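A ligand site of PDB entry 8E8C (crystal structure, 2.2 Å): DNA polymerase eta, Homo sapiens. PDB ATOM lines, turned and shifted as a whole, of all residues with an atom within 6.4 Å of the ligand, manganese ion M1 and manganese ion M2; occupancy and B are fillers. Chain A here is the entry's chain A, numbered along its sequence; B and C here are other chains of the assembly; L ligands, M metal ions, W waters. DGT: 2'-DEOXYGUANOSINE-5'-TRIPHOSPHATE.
An oxygen (O1G) of the ligand lies within hydrogen-bond range of the side-chain hydroxyl of Tyr 55 (2.7 Å). O3' of the ligand lies within hydrogen-bond range of N of Phe 21. N of Cys 19 is in hydrogen-bond range of O1G of the ligand (2.8 Å). An oxygen (O3') of the ligand is in hydrogen-bond range of the backbone NH of Phe 20 (3.2 Å). NZ of Lys 234 is in salt-bridge range of O1G of the ligand (3.3 Å). The guanidinium group (NH2) of Arg 64 sits at hydrogen-bond distance from an oxygen (O6) of the ligand, 2.6 Å away. O4' of DA 5 of chain B is in hydrogen-bond range of a nitrogen (N2) of the ligand, at 3.1 Å. O2 of DT 4 of chain B is in hydrogen-bond range of a nitrogen (N1) of the ligand (2.5 Å). A nitrogen (N1) of the ligand is in hydrogen-bond range of N3 of DA 5 of chain B (3.4 Å). The side-chain amide oxygen of Gln 41 sits at hydrogen-bond distance from a nitrogen (N2) of the ligand. NH1 of Arg 58 lies within salt-bridge range of O3G of the ligand, at 2.9 Å.
OD2 of Asp 16 lies close to NZ of Lys 234 (2.7 Å). The backbone NH of Asp 118 lies close to the side-chain hydroxyl of Ser 116. O4 of U 8 of chain C sits at hydrogen-bond distance from NH2 of Arg 64, at 2.8 Å. N3 of U 8 of chain C sits close to N1 of DA 5 of chain B, at 2.6 Å. The guanidinium group of Arg 58 sits at hydrogen-bond distance from the side-chain hydroxyl of Tyr 55 (3.2 Å). NZ of Lys 227 is in salt-bridge range of OP1 of U 8 of chain C (3.8 Å). O3' of U 8 of chain C lies close to the side-chain hydroxyl (OG) of Ser 116, 3.1 Å away. OE2 of Glu 119 is in hydrogen-bond range of OG of Ser 116, 3.2 Å away.
Merely in contact with the ligand: Asp 18 (3.2 Å), Ile 51 (3.4 Å), Ala 52 (3.6 Å) and Ile 117 (3.8 Å). 18 residues have an atom within 4 Å of the ligand: Asp 16, Met 17, Asp 18, Cys 19, Phe 20, Phe 21, Gln 41, Ile 51, Ala 52, Tyr 55, Arg 58, Arg 64, Ile 117, Asp 118, Lys 234, DT 4 of chain B, DA 5 of chain B and U 8 of chain C. The nearest printed residue that does not touch the ligand is Leu 92 (4.2 Å).
Of the 28 residues printed, 3 come within 4 Å of manganese ion M1. The nearest printed residue that does not touch manganese ion M1 is Lys 234 (4.1 Å).
OG of Ser 116 touches manganese ion M2 (3.99 Å). OE2 of Glu 119 touches manganese ion M2 (3.0 Å). Within 4 Å of manganese ion M2: Asp 16, Ser 116, Asp 118, Glu 119 and U 8 of chain C.
Manganese ion M1 is bound by an oxygen (O2B) of the ligand (2.0 Å), the side-chain carboxylate of Asp 118 (2.2 Å), an oxygen (O2G) of the ligand (2.2 Å), the side-chain carboxylate of Asp 16 (2.2 Å), the backbone carbonyl oxygen of Met 17 (2.3 Å) and an oxygen (O1A) of the ligand (2.5 Å). Manganese ion M1 has six donor atoms within binding distance.
O1A of the ligand binds manganese ion M2 (2.2 Å). The side-chain carboxylate (OD1) of Asp 118 binds manganese ion M2 (2.4 Å). Water W1 is bound to manganese ion M2. Manganese ion M2 is bound by OD1 of Asp 16, 2.4 Å away. Manganese ion M2 is bound by O3' of U 8 of chain C (2.6 Å). Manganese ion M2 has five donor atoms within binding distance.
Water W1 bridges NZ of Lys 227 (3.0 Å) and O2A of the ligand (3.4 Å). Water W2 lies within hydrogen-bond range of an oxygen (O2A) of the ligand, N1 of U 8 of chain C and the guanidinium group (NE) of Arg 64.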
ATOM      1  N   VAL A  15     -37.788  13.239  12.047  1.00  0.00           N
ATOM      2  CA  VAL A  15     -36.584  12.445  11.878  1.00  0.00           C
ATOM      3  C   VAL A  15     -35.701  13.109  10.832  1.00  0.00           C
ATOM      4  O   VAL A  15     -36.168  13.493   9.752  1.00  0.00           O
ATOM      5  CB  VAL A  15     -36.917  11.003  11.504  1.00  0.00           C
ATOM      6  CG1 VAL A  15     -35.632  10.193  11.272  1.00  0.00           C
ATOM      7  CG2 VAL A  15     -37.758  10.385  12.611  1.00  0.00           C
ATOM      8  N   ASP A  16     -34.413  13.239  11.153  1.00  0.00           N
ATOM      9  CA  ASP A  16     -33.447  13.930  10.332  1.00  0.00           C
ATOM     10  C   ASP A  16     -32.169  13.107  10.248  1.00  0.00           C
ATOM     11  O   ASP A  16     -31.523  12.839  11.270  1.00  0.00           O
ATOM     12  CB  ASP A  16     -33.132  15.276  10.947  1.00  0.00           C
ATOM     13  CG  ASP A  16     -32.426  16.153  10.019  1.00  0.00           C
ATOM     14  OD1 ASP A  16     -33.096  16.854   9.231  1.00  0.00           O
ATOM     15  OD2 ASP A  16     -31.189  16.091  10.047  1.00  0.00           O
ATOM     16  N   MET A  17     -31.787  12.709   9.029  1.00  0.00           N
ATOM     17  CA  MET A  17     -30.522  12.002   8.841  1.00  0.00           C
ATOM     18  C   MET A  17     -29.343  12.915   9.158  1.00  0.00           C
ATOM     19  O   MET A  17     -29.237  14.007   8.615  1.00  0.00           O
ATOM     20  CB  MET A  17     -30.418  11.465   7.407  1.00  0.00           C
ATOM     21  CG  MET A  17     -31.740  10.923   6.891  1.00  0.00           C
ATOM     22  SD  MET A  17     -32.293   9.544   7.930  1.00  0.00           S
ATOM     23  CE  MET A  17     -30.748   8.627   8.079  1.00  0.00           C
ATOM     24  N   ASP A  18     -28.446  12.447  10.028  1.00  0.00           N
ATOM     25  CA  ASP A  18     -27.225  13.175  10.330  1.00  0.00           C
ATOM     26  C   ASP A  18     -26.363  13.305   9.081  1.00  0.00           C
ATOM     27  O   ASP A  18     -26.100  12.303   8.408  1.00  0.00           O
ATOM     28  CB  ASP A  18     -26.432  12.451  11.419  1.00  0.00           C
ATOM     29  CG  ASP A  18     -27.236  12.249  12.690  1.00  0.00           C
ATOM     30  OD1 ASP A  18     -28.145  13.044  12.976  1.00  0.00           O
ATOM     31  OD2 ASP A  18     -26.942  11.291  13.414  1.00  0.00           O
ATOM     32  N   CYS A  19     -25.877  14.526   8.809  1.00  0.00           N
ATOM     33  CA  CYS A  19     -25.026  14.856   7.668  1.00  0.00           C
ATOM     34  C   CYS A  19     -25.229  13.897   6.499  1.00  0.00           C
ATOM     35  O   CYS A  19     -24.352  13.083   6.197  1.00  0.00           O
ATOM     36  CB  CYS A  19     -23.547  14.876   8.093  1.00  0.00           C
ATOM     37  SG  CYS A  19     -22.895  13.379   8.945  1.00  0.00           S
ATOM     38  N   PHE A  20     -26.395  13.994   5.858  1.00  0.00           N
ATOM     39  CA  PHE A  20     -26.912  12.887   5.062  1.00  0.00           C
ATOM     40  C   PHE A  20     -26.039  12.584   3.849  1.00  0.00           C
ATOM     41  O   PHE A  20     -25.723  11.403   3.572  1.00  0.00           O
ATOM     42  CB  PHE A  20     -28.341  13.183   4.647  1.00  0.00           C
ATOM     43  CG  PHE A  20     -28.981  12.065   3.903  1.00  0.00           C
ATOM     44  CD1 PHE A  20     -28.867  10.772   4.380  1.00  0.00           C
ATOM     45  CD2 PHE A  20     -29.665  12.284   2.720  1.00  0.00           C
ATOM     46  CE1 PHE A  20     -29.446   9.703   3.683  1.00  0.00           C
ATOM     47  CE2 PHE A  20     -30.255  11.231   2.025  1.00  0.00           C
ATOM     48  CZ  PHE A  20     -30.136   9.940   2.515  1.00  0.00           C
ATOM     49  N   PHE A  21     -25.668  13.608   3.073  1.00  0.00           N
ATOM     50  CA  PHE A  21     -24.846  13.344   1.886  1.00  0.00           C
ATOM     51  C   PHE A  21     -23.509  12.707   2.282  1.00  0.00           C
ATOM     52  O   PHE A  21     -23.022  11.787   1.602  1.00  0.00           O
ATOM     53  CB  PHE A  21     -24.629  14.627   1.085  1.00  0.00           C
ATOM     54  CG  PHE A  21     -25.853  15.108   0.311  1.00  0.00           C
ATOM     55  CD1 PHE A  21     -27.120  14.751   0.669  1.00  0.00           C
ATOM     56  CD2 PHE A  21     -25.688  15.916  -0.797  1.00  0.00           C
ATOM     57  CE1 PHE A  21     -28.240  15.189  -0.057  1.00  0.00           C
ATOM     58  CE2 PHE A  21     -26.794  16.363  -1.538  1.00  0.00           C
ATOM     59  CZ  PHE A  21     -28.070  15.988  -1.166  1.00  0.00           C
ATOM     60  N   VAL A  22     -22.920  13.154   3.399  1.00  0.00           N
ATOM     61  CA  VAL A  22     -21.682  12.580   3.888  1.00  0.00           C
ATOM     62  C   VAL A  22     -21.860  11.110   4.243  1.00  0.00           C
ATOM     63  O   VAL A  22     -21.043  10.262   3.877  1.00  0.00           O
ATOM     64  CB  VAL A  22     -21.157  13.385   5.084  1.00  0.00           C
ATOM     65  CG1 VAL A  22     -20.003  12.643   5.726  1.00  0.00           C
ATOM     66  CG2 VAL A  22     -20.713  14.743   4.638  1.00  0.00           C
ATOM     67  N   GLN A  41     -19.702  20.294  -4.144  1.00  0.00           N
ATOM     68  CA  GLN A  41     -20.204  20.437  -5.514  1.00  0.00           C
ATOM     69  C   GLN A  41     -19.183  21.244  -6.305  1.00  0.00           C
ATOM     70  O   GLN A  41     -18.797  22.338  -5.879  1.00  0.00           O
ATOM     71  CB  GLN A  41     -21.562  21.158  -5.553  1.00  0.00           C
ATOM     72  CG  GLN A  41     -22.710  20.398  -4.914  1.00  0.00           C
ATOM     73  CD  GLN A  41     -24.072  21.065  -5.102  1.00  0.00           C
ATOM     74  OE1 GLN A  41     -25.053  20.397  -5.444  1.00  0.00           O
ATOM     75  NE2 GLN A  41     -24.152  22.373  -4.859  1.00  0.00           N
ATOM     76  N   ILE A  51     -21.435  21.228   0.898  1.00  0.00           N
ATOM     77  CA  ILE A  51     -22.856  21.203   1.197  1.00  0.00           C
ATOM     78  C   ILE A  51     -23.223  20.266   2.350  1.00  0.00           C
ATOM     79  O   ILE A  51     -24.396  20.249   2.750  1.00  0.00           O
ATOM     80  CB  ILE A  51     -23.696  20.841  -0.052  1.00  0.00           C
ATOM     81  CG1 ILE A  51     -23.172  19.578  -0.728  1.00  0.00           C
ATOM     82  CG2 ILE A  51     -23.715  22.023  -1.043  1.00  0.00           C
ATOM     83  CD1 ILE A  51     -24.052  19.100  -1.816  1.00  0.00           C
ATOM     84  N   ALA A  52     -22.284  19.489   2.883  1.00  0.00           N
ATOM     85  CA  ALA A  52     -22.572  18.557   3.978  1.00  0.00           C
ATOM     86  C   ALA A  52     -21.269  18.223   4.700  1.00  0.00           C
ATOM     87  O   ALA A  52     -20.230  18.026   4.070  1.00  0.00           O
ATOM     88  CB  ALA A  52     -23.242  17.278   3.475  1.00  0.00           C
ATOM     89  N   VAL A  53     -21.324  18.146   6.033  1.00  0.00           N
ATOM     90  CA  VAL A  53     -20.121  18.052   6.843  1.00  0.00           C
ATOM     91  C   VAL A  53     -20.338  17.034   7.950  1.00  0.00           C
ATOM     92  O   VAL A  53     -21.291  17.158   8.721  1.00  0.00           O
ATOM     93  CB  VAL A  53     -19.742  19.415   7.441  1.00  0.00           C
ATOM     94  CG1 VAL A  53     -18.317  19.383   7.952  1.00  0.00           C
ATOM     95  CG2 VAL A  53     -19.890  20.495   6.397  1.00  0.00           C
ATOM     96  N   TYR A  55     -19.634  15.194  11.592  1.00  0.00           N
ATOM     97  CA  TYR A  55     -19.530  15.883  12.869  1.00  0.00           C
ATOM     98  C   TYR A  55     -18.083  16.023  13.316  1.00  0.00           C
ATOM     99  O   TYR A  55     -17.706  17.028  13.933  1.00  0.00           O
ATOM    100  CB  TYR A  55     -20.376  15.171  13.925  1.00  0.00           C
ATOM    101  CG  TYR A  55     -21.840  15.572  13.747  1.00  0.00           C
ATOM    102  CD1 TYR A  55     -22.601  15.035  12.718  1.00  0.00           C
ATOM    103  CD2 TYR A  55     -22.422  16.543  14.550  1.00  0.00           C
ATOM    104  CE1 TYR A  55     -23.941  15.409  12.532  1.00  0.00           C
ATOM    105  CE2 TYR A  55     -23.742  16.942  14.368  1.00  0.00           C
ATOM    106  CZ  TYR A  55     -24.496  16.371  13.365  1.00  0.00           C
ATOM    107  OH  TYR A  55     -25.823  16.765  13.178  1.00  0.00           O
ATOM    108  N   ARG A  58     -17.074  19.085  11.466  1.00  0.00           N
ATOM    109  CA  ARG A  58     -17.666  20.246  12.144  1.00  0.00           C
ATOM    110  C   ARG A  58     -16.899  20.655  13.403  1.00  0.00           C
ATOM    111  O   ARG A  58     -16.861  21.842  13.753  1.00  0.00           O
ATOM    112  CB  ARG A  58     -19.127  19.978  12.525  1.00  0.00           C
ATOM    113  CG  ARG A  58     -20.087  19.880  11.352  1.00  0.00           C
ATOM    114  CD  ARG A  58     -21.476  19.557  11.830  1.00  0.00           C
ATOM    115  NE  ARG A  58     -22.282  18.995  10.745  1.00  0.00           N
ATOM    116  CZ  ARG A  58     -23.597  18.875  10.780  1.00  0.00           C
ATOM    117  NH1 ARG A  58     -24.297  19.223  11.859  1.00  0.00           N
ATOM    118  NH2 ARG A  58     -24.228  18.423   9.700  1.00  0.00           N
ATOM    119  N   ARG A  64     -21.301  24.126   6.186  1.00  0.00           N
ATOM    120  CA  ARG A  64     -21.900  24.147   4.846  1.00  0.00           C
ATOM    121  C   ARG A  64     -21.738  25.549   4.257  1.00  0.00           C
ATOM    122  O   ARG A  64     -21.588  26.561   4.960  1.00  0.00           O
ATOM    123  CB  ARG A  64     -23.377  23.699   4.905  1.00  0.00           C
ATOM    124  CG  ARG A  64     -24.473  24.769   4.751  1.00  0.00           C
ATOM    125  CD  ARG A  64     -25.841  24.127   4.630  1.00  0.00           C
ATOM    126  NE  ARG A  64     -26.510  24.477   3.390  1.00  0.00           N
ATOM    127  CZ  ARG A  64     -27.224  25.576   3.205  1.00  0.00           C
ATOM    128  NH1 ARG A  64     -27.361  26.450   4.195  1.00  0.00           N
ATOM    129  NH2 ARG A  64     -27.791  25.820   2.038  1.00  0.00           N
ATOM    130  N   LEU A  92     -27.984  15.014  -8.281  1.00  0.00           N
ATOM    131  CA  LEU A  92     -28.136  14.566  -6.901  1.00  0.00           C
ATOM    132  C   LEU A  92     -28.835  13.209  -6.799  1.00  0.00           C
ATOM    133  O   LEU A  92     -29.386  12.883  -5.748  1.00  0.00           O
ATOM    134  CB  LEU A  92     -28.871  15.629  -6.082  1.00  0.00           C
ATOM    135  CG  LEU A  92     -28.212  17.004  -6.128  1.00  0.00           C
ATOM    136  CD1 LEU A  92     -29.052  18.042  -5.397  1.00  0.00           C
ATOM    137  CD2 LEU A  92     -26.836  16.948  -5.520  1.00  0.00           C
ATOM    138  N   SER A 116     -37.928  17.190   3.455  1.00  0.00           N
ATOM    139  CA  SER A 116     -36.808  17.474   2.562  1.00  0.00           C
ATOM    140  C   SER A 116     -36.113  16.153   2.282  1.00  0.00           C
ATOM    141  O   SER A 116     -36.470  15.126   2.864  1.00  0.00           O
ATOM    142  CB  SER A 116     -35.820  18.475   3.166  1.00  0.00           C
ATOM    143  OG  SER A 116     -34.890  17.782   3.983  1.00  0.00           O
ATOM    144  N   ILE A 117     -35.061  16.213   1.455  1.00  0.00           N
ATOM    145  CA  ILE A 117     -34.409  14.982   1.010  1.00  0.00           C
ATOM    146  C   ILE A 117     -34.015  14.108   2.178  1.00  0.00           C
ATOM    147  O   ILE A 117     -33.981  12.882   2.073  1.00  0.00           O
ATOM    148  CB  ILE A 117     -33.191  15.314   0.143  1.00  0.00           C
ATOM    149  CG1 ILE A 117     -32.675  14.056  -0.524  1.00  0.00           C
ATOM    150  CG2 ILE A 117     -32.086  15.913   0.982  1.00  0.00           C
ATOM    151  CD1 ILE A 117     -32.093  14.360  -1.878  1.00  0.00           C
ATOM    152  N   ASP A 118     -33.725  14.720   3.334  1.00  0.00           N
ATOM    153  CA  ASP A 118     -33.193  13.950   4.438  1.00  0.00           C
ATOM    154  C   ASP A 118     -34.016  14.079   5.708  1.00  0.00           C
ATOM    155  O   ASP A 118     -33.541  13.689   6.779  1.00  0.00           O
ATOM    156  CB  ASP A 118     -31.762  14.371   4.739  1.00  0.00           C
ATOM    157  CG  ASP A 118     -31.706  15.561   5.635  1.00  0.00           C
ATOM    158  OD1 ASP A 118     -32.437  16.548   5.367  1.00  0.00           O
ATOM    159  OD2 ASP A 118     -30.947  15.472   6.628  1.00  0.00           O
ATOM    160  N   GLU A 119     -35.228  14.634   5.630  1.00  0.00           N
ATOM    161  CA  GLU A 119     -35.991  14.673   6.863  1.00  0.00           C
ATOM    162  C   GLU A 119     -37.466  14.530   6.571  1.00  0.00           C
ATOM    163  O   GLU A 119     -37.982  15.022   5.559  1.00  0.00           O
ATOM    164  CB  GLU A 119     -35.704  15.943   7.666  1.00  0.00           C
ATOM    165  CG  GLU A 119     -36.534  17.131   7.333  1.00  0.00           C
ATOM    166  CD  GLU A 119     -35.858  18.420   7.742  1.00  0.00           C
ATOM    167  OE1 GLU A 119     -35.880  18.775   8.934  1.00  0.00           O
ATOM    168  OE2 GLU A 119     -35.299  19.096   6.858  1.00  0.00           O
ATOM    169  N   SER A 216     -30.935  11.605  13.813  1.00  0.00           N
ATOM    170  CA  SER A 216     -31.493  12.141  15.040  1.00  0.00           C
ATOM    171  C   SER A 216     -32.994  12.307  14.859  1.00  0.00           C
ATOM    172  O   SER A 216     -33.515  12.281  13.742  1.00  0.00           O
ATOM    173  CB  SER A 216     -30.845  13.476  15.375  1.00  0.00           C
ATOM    174  OG  SER A 216     -29.443  13.331  15.550  1.00  0.00           O
ATOM    175  N   LYS A 227     -39.293  19.406  15.421  1.00  0.00           N
ATOM    176  CA  LYS A 227     -38.120  19.868  14.686  1.00  0.00           C
ATOM    177  C   LYS A 227     -37.120  20.538  15.618  1.00  0.00           C
ATOM    178  O   LYS A 227     -35.918  20.281  15.546  1.00  0.00           O
ATOM    179  CB  LYS A 227     -38.568  20.822  13.576  1.00  0.00           C
ATOM    180  CG  LYS A 227     -37.442  21.505  12.799  1.00  0.00           C
ATOM    181  CD  LYS A 227     -36.718  20.537  11.870  1.00  0.00           C
ATOM    182  CE  LYS A 227     -35.716  21.266  10.985  1.00  0.00           C
ATOM    183  NZ  LYS A 227     -34.638  20.336  10.579  1.00  0.00           N
ATOM    184  N   LYS A 234     -27.745  16.173  18.808  1.00  0.00           N
ATOM    185  CA  LYS A 234     -27.250  15.586  17.588  1.00  0.00           C
ATOM    186  C   LYS A 234     -25.769  15.277  17.776  1.00  0.00           C
ATOM    187  O   LYS A 234     -25.099  15.924  18.584  1.00  0.00           O
ATOM    188  CB  LYS A 234     -27.454  16.544  16.402  1.00  0.00           C
ATOM    189  CG  LYS A 234     -28.935  16.851  16.047  1.00  0.00           C
ATOM    190  CD  LYS A 234     -29.124  17.176  14.533  1.00  0.00           C
ATOM    191  CE  LYS A 234     -29.023  15.882  13.675  1.00  0.00           C
ATOM    192  NZ  LYS A 234     -29.783  15.751  12.377  1.00  0.00           N
ATOM    193  N   PRO A 235     -25.235  14.257  17.096  1.00  0.00           N
ATOM    194  CA  PRO A 235     -25.887  13.283  16.213  1.00  0.00           C
ATOM    195  C   PRO A 235     -26.335  12.014  16.902  1.00  0.00           C
ATOM    196  O   PRO A 235     -26.031  11.759  18.071  1.00  0.00           O
ATOM    197  CB  PRO A 235     -24.786  12.983  15.192  1.00  0.00           C
ATOM    198  CG  PRO A 235     -23.518  13.022  16.018  1.00  0.00           C
ATOM    199  CD  PRO A 235     -23.766  14.069  17.095  1.00  0.00           C
ATOM    200  P    DT B   4     -22.778  30.283  -5.555  1.00  0.00           P
ATOM    201  OP1  DT B   4     -22.042  30.654  -6.814  1.00  0.00           O
ATOM    202  OP2  DT B   4     -23.923  31.209  -5.186  1.00  0.00           O
ATOM    203  O5'  DT B   4     -23.410  28.821  -5.778  1.00  0.00           O
ATOM    204  C5'  DT B   4     -22.572  27.797  -6.351  1.00  0.00           C
ATOM    205  C4'  DT B   4     -23.328  26.495  -6.397  1.00  0.00           C
ATOM    206  O4'  DT B   4     -23.837  26.181  -5.074  1.00  0.00           O
ATOM    207  C3'  DT B   4     -24.539  26.485  -7.316  1.00  0.00           C
ATOM    208  O3'  DT B   4     -24.770  25.159  -7.774  1.00  0.00           O
ATOM    209  C2'  DT B   4     -25.674  26.815  -6.364  1.00  0.00           C
ATOM    210  C1'  DT B   4     -25.240  26.024  -5.147  1.00  0.00           C
ATOM    211  N1   DT B   4     -25.808  26.527  -3.889  1.00  0.00           N
ATOM    212  C2   DT B   4     -26.347  25.617  -3.020  1.00  0.00           C
ATOM    213  O2   DT B   4     -26.364  24.412  -3.247  1.00  0.00           O
ATOM    214  N3   DT B   4     -26.855  26.152  -1.863  1.00  0.00           N
ATOM    215  C4   DT B   4     -26.872  27.493  -1.511  1.00  0.00           C
ATOM    216  O4   DT B   4     -27.363  27.819  -0.440  1.00  0.00           O
ATOM    217  C5   DT B   4     -26.287  28.391  -2.476  1.00  0.00           C
ATOM    218  C7   DT B   4     -26.275  29.860  -2.177  1.00  0.00           C
ATOM    219  C6   DT B   4     -25.788  27.872  -3.610  1.00  0.00           C
ATOM    220  P    DA B   5     -25.779  24.878  -8.962  1.00  0.00           P
ATOM    221  OP1  DA B   5     -25.052  24.019  -9.924  1.00  0.00           O
ATOM    222  OP2  DA B   5     -26.396  26.158  -9.391  1.00  0.00           O
ATOM    223  O5'  DA B   5     -26.888  23.985  -8.270  1.00  0.00           O
ATOM    224  C5'  DA B   5     -26.465  22.949  -7.435  1.00  0.00           C
ATOM    225  C4'  DA B   5     -27.580  21.990  -7.094  1.00  0.00           C
ATOM    226  O4'  DA B   5     -28.151  22.324  -5.807  1.00  0.00           O
ATOM    227  C3'  DA B   5     -28.754  21.969  -8.047  1.00  0.00           C
ATOM    228  O3'  DA B   5     -29.324  20.672  -7.991  1.00  0.00           O
ATOM    229  C2'  DA B   5     -29.683  23.029  -7.441  1.00  0.00           C
ATOM    230  C1'  DA B   5     -29.476  22.776  -5.944  1.00  0.00           C
ATOM    231  N9   DA B   5     -29.601  23.938  -5.109  1.00  0.00           N
ATOM    232  C8   DA B   5     -29.251  25.230  -5.421  1.00  0.00           C
ATOM    233  N7   DA B   5     -29.433  26.075  -4.433  1.00  0.00           N
ATOM    234  C5   DA B   5     -29.922  25.281  -3.404  1.00  0.00           C
ATOM    235  C6   DA B   5     -30.325  25.577  -2.079  1.00  0.00           C
ATOM    236  N6   DA B   5     -30.291  26.810  -1.553  1.00  0.00           N
ATOM    237  N1   DA B   5     -30.758  24.550  -1.327  1.00  0.00           N
ATOM    238  C2   DA B   5     -30.792  23.318  -1.853  1.00  0.00           C
ATOM    239  N3   DA B   5     -30.453  22.928  -3.073  1.00  0.00           N
ATOM    240  C4   DA B   5     -30.023  23.963  -3.803  1.00  0.00           C
ATOM    241  P    DT B   6     -30.560  20.257  -8.936  1.00  0.00           P
ATOM    242  OP1  DT B   6     -30.911  18.868  -8.586  1.00  0.00           O
ATOM    243  OP2  DT B   6     -30.215  20.580 -10.347  1.00  0.00           O
ATOM    244  O5'  DT B   6     -31.712  21.246  -8.506  1.00  0.00           O
ATOM    245  C5'  DT B   6     -32.941  20.760  -8.171  1.00  0.00           C
ATOM    246  C4'  DT B   6     -33.102  20.713  -6.670  1.00  0.00           C
ATOM    247  O4'  DT B   6     -32.653  21.969  -6.110  1.00  0.00           O
ATOM    248  C3'  DT B   6     -34.548  20.559  -6.252  1.00  0.00           C
ATOM    249  O3'  DT B   6     -34.812  19.201  -5.907  1.00  0.00           O
ATOM    250  C2'  DT B   6     -34.735  21.544  -5.073  1.00  0.00           C
ATOM    251  C1'  DT B   6     -33.366  22.195  -4.916  1.00  0.00           C
ATOM    252  N1   DT B   6     -33.385  23.659  -4.651  1.00  0.00           N
ATOM    253  C2   DT B   6     -33.623  24.085  -3.373  1.00  0.00           C
ATOM    254  O2   DT B   6     -33.880  23.326  -2.460  1.00  0.00           O
ATOM    255  N3   DT B   6     -33.559  25.429  -3.200  1.00  0.00           N
ATOM    256  C4   DT B   6     -33.269  26.376  -4.147  1.00  0.00           C
ATOM    257  O4   DT B   6     -33.244  27.571  -3.876  1.00  0.00           O
ATOM    258  C5   DT B   6     -33.013  25.869  -5.463  1.00  0.00           C
ATOM    259  C7   DT B   6     -32.697  26.820  -6.586  1.00  0.00           C
ATOM    260  C6   DT B   6     -33.076  24.539  -5.654  1.00  0.00           C
ATOM    261  P     U C   8     -33.331  24.417   8.267  1.00  0.00           P
ATOM    262  OP1   U C   8     -33.478  23.819   9.639  1.00  0.00           O
ATOM    263  OP2   U C   8     -32.230  25.449   8.139  1.00  0.00           O
ATOM    264  O5'   U C   8     -32.993  23.199   7.240  1.00  0.00           O
ATOM    265  C5'   U C   8     -34.076  22.342   6.797  1.00  0.00           C
ATOM    266  C4'   U C   8     -33.769  21.775   5.427  1.00  0.00           C
ATOM    267  O4'   U C   8     -33.653  22.873   4.494  1.00  0.00           O
ATOM    268  C3'   U C   8     -32.448  21.017   5.311  1.00  0.00           C
ATOM    269  O3'   U C   8     -32.720  19.632   5.217  1.00  0.00           O
ATOM    270  C2'   U C   8     -31.872  21.389   3.941  1.00  0.00           C
ATOM    271  O2'   U C   8     -31.973  20.236   3.138  1.00  0.00           O
ATOM    272  C1'   U C   8     -32.802  22.489   3.436  1.00  0.00           C
ATOM    273  N1    U C   8     -32.106  23.699   2.973  1.00  0.00           N
ATOM    274  C2    U C   8     -31.759  23.759   1.641  1.00  0.00           C
ATOM    275  O2    U C   8     -31.989  22.843   0.860  1.00  0.00           O
ATOM    276  N3    U C   8     -31.146  24.913   1.253  1.00  0.00           N
ATOM    277  C4    U C   8     -30.842  26.005   2.034  1.00  0.00           C
ATOM    278  O4    U C   8     -30.280  26.980   1.533  1.00  0.00           O
ATOM    279  C5    U C   8     -31.235  25.879   3.407  1.00  0.00           C
ATOM    280  C6    U C   8     -31.846  24.748   3.814  1.00  0.00           C
HETATM  281  PG  DGT L   1     -27.382  17.634  10.076  1.00  0.00           P
HETATM  282  O1G DGT L   1     -26.954  16.316  10.712  1.00  0.00           O
HETATM  283  O2G DGT L   1     -28.866  17.571   9.736  1.00  0.00           O
HETATM  284  O3G DGT L   1     -27.020  18.865  10.927  1.00  0.00           O
HETATM  285  O3B DGT L   1     -26.649  17.646   8.648  1.00  0.00           O
HETATM  286  PB  DGT L   1     -27.300  17.558   7.192  1.00  0.00           P
HETATM  287  O1B DGT L   1     -26.169  17.541   6.108  1.00  0.00           O
HETATM  288  O2B DGT L   1     -28.255  16.420   7.068  1.00  0.00           O
HETATM  289  O3A DGT L   1     -28.010  18.974   7.099  1.00  0.00           O
HETATM  290  PA  DGT L   1     -29.487  19.371   6.661  1.00  0.00           P
HETATM  291  O1A DGT L   1     -30.423  18.373   7.385  1.00  0.00           O
HETATM  292  O2A DGT L   1     -29.732  20.805   7.024  1.00  0.00           O
HETATM  293  O5' DGT L   1     -29.560  19.076   5.046  1.00  0.00           O
HETATM  294  C5' DGT L   1     -29.825  17.785   4.442  1.00  0.00           C
HETATM  295  C4' DGT L   1     -28.895  17.455   3.296  1.00  0.00           C
HETATM  296  O4' DGT L   1     -29.273  18.220   2.125  1.00  0.00           O
HETATM  297  C3' DGT L   1     -27.416  17.746   3.533  1.00  0.00           C
HETATM  298  O3' DGT L   1     -26.758  16.571   4.007  1.00  0.00           O
HETATM  299  C2' DGT L   1     -26.903  18.091   2.144  1.00  0.00           C
HETATM  300  C1' DGT L   1     -28.116  18.659   1.421  1.00  0.00           C
HETATM  301  N9  DGT L   1     -28.145  20.134   1.378  1.00  0.00           N
HETATM  302  C8  DGT L   1     -28.307  21.025   2.397  1.00  0.00           C
HETATM  303  N7  DGT L   1     -28.207  22.295   2.001  1.00  0.00           N
HETATM  304  C5  DGT L   1     -27.950  22.193   0.635  1.00  0.00           C
HETATM  305  C6  DGT L   1     -27.671  23.171  -0.351  1.00  0.00           C
HETATM  306  O6  DGT L   1     -27.666  24.379  -0.106  1.00  0.00           O
HETATM  307  N1  DGT L   1     -27.394  22.769  -1.608  1.00  0.00           N
HETATM  308  C2  DGT L   1     -27.413  21.399  -1.860  1.00  0.00           C
HETATM  309  N2  DGT L   1     -27.139  21.042  -3.116  1.00  0.00           N
HETATM  310  N3  DGT L   1     -27.681  20.445  -0.973  1.00  0.00           N
HETATM  311  C4  DGT L   1     -27.921  20.897   0.256  1.00  0.00           C
HETATM  312 MN    MN M   1     -29.820  16.189   8.333  1.00  0.00          MN
HETATM  313 MN    MN M   2     -32.568  18.002   7.216  1.00  0.00          MN
HETATM  314  O   HOH W   1     -32.167  19.450   9.034  1.00  0.00           O
HETATM  315  O   HOH W   2     -29.415  23.497   5.064  1.00  0.00           O
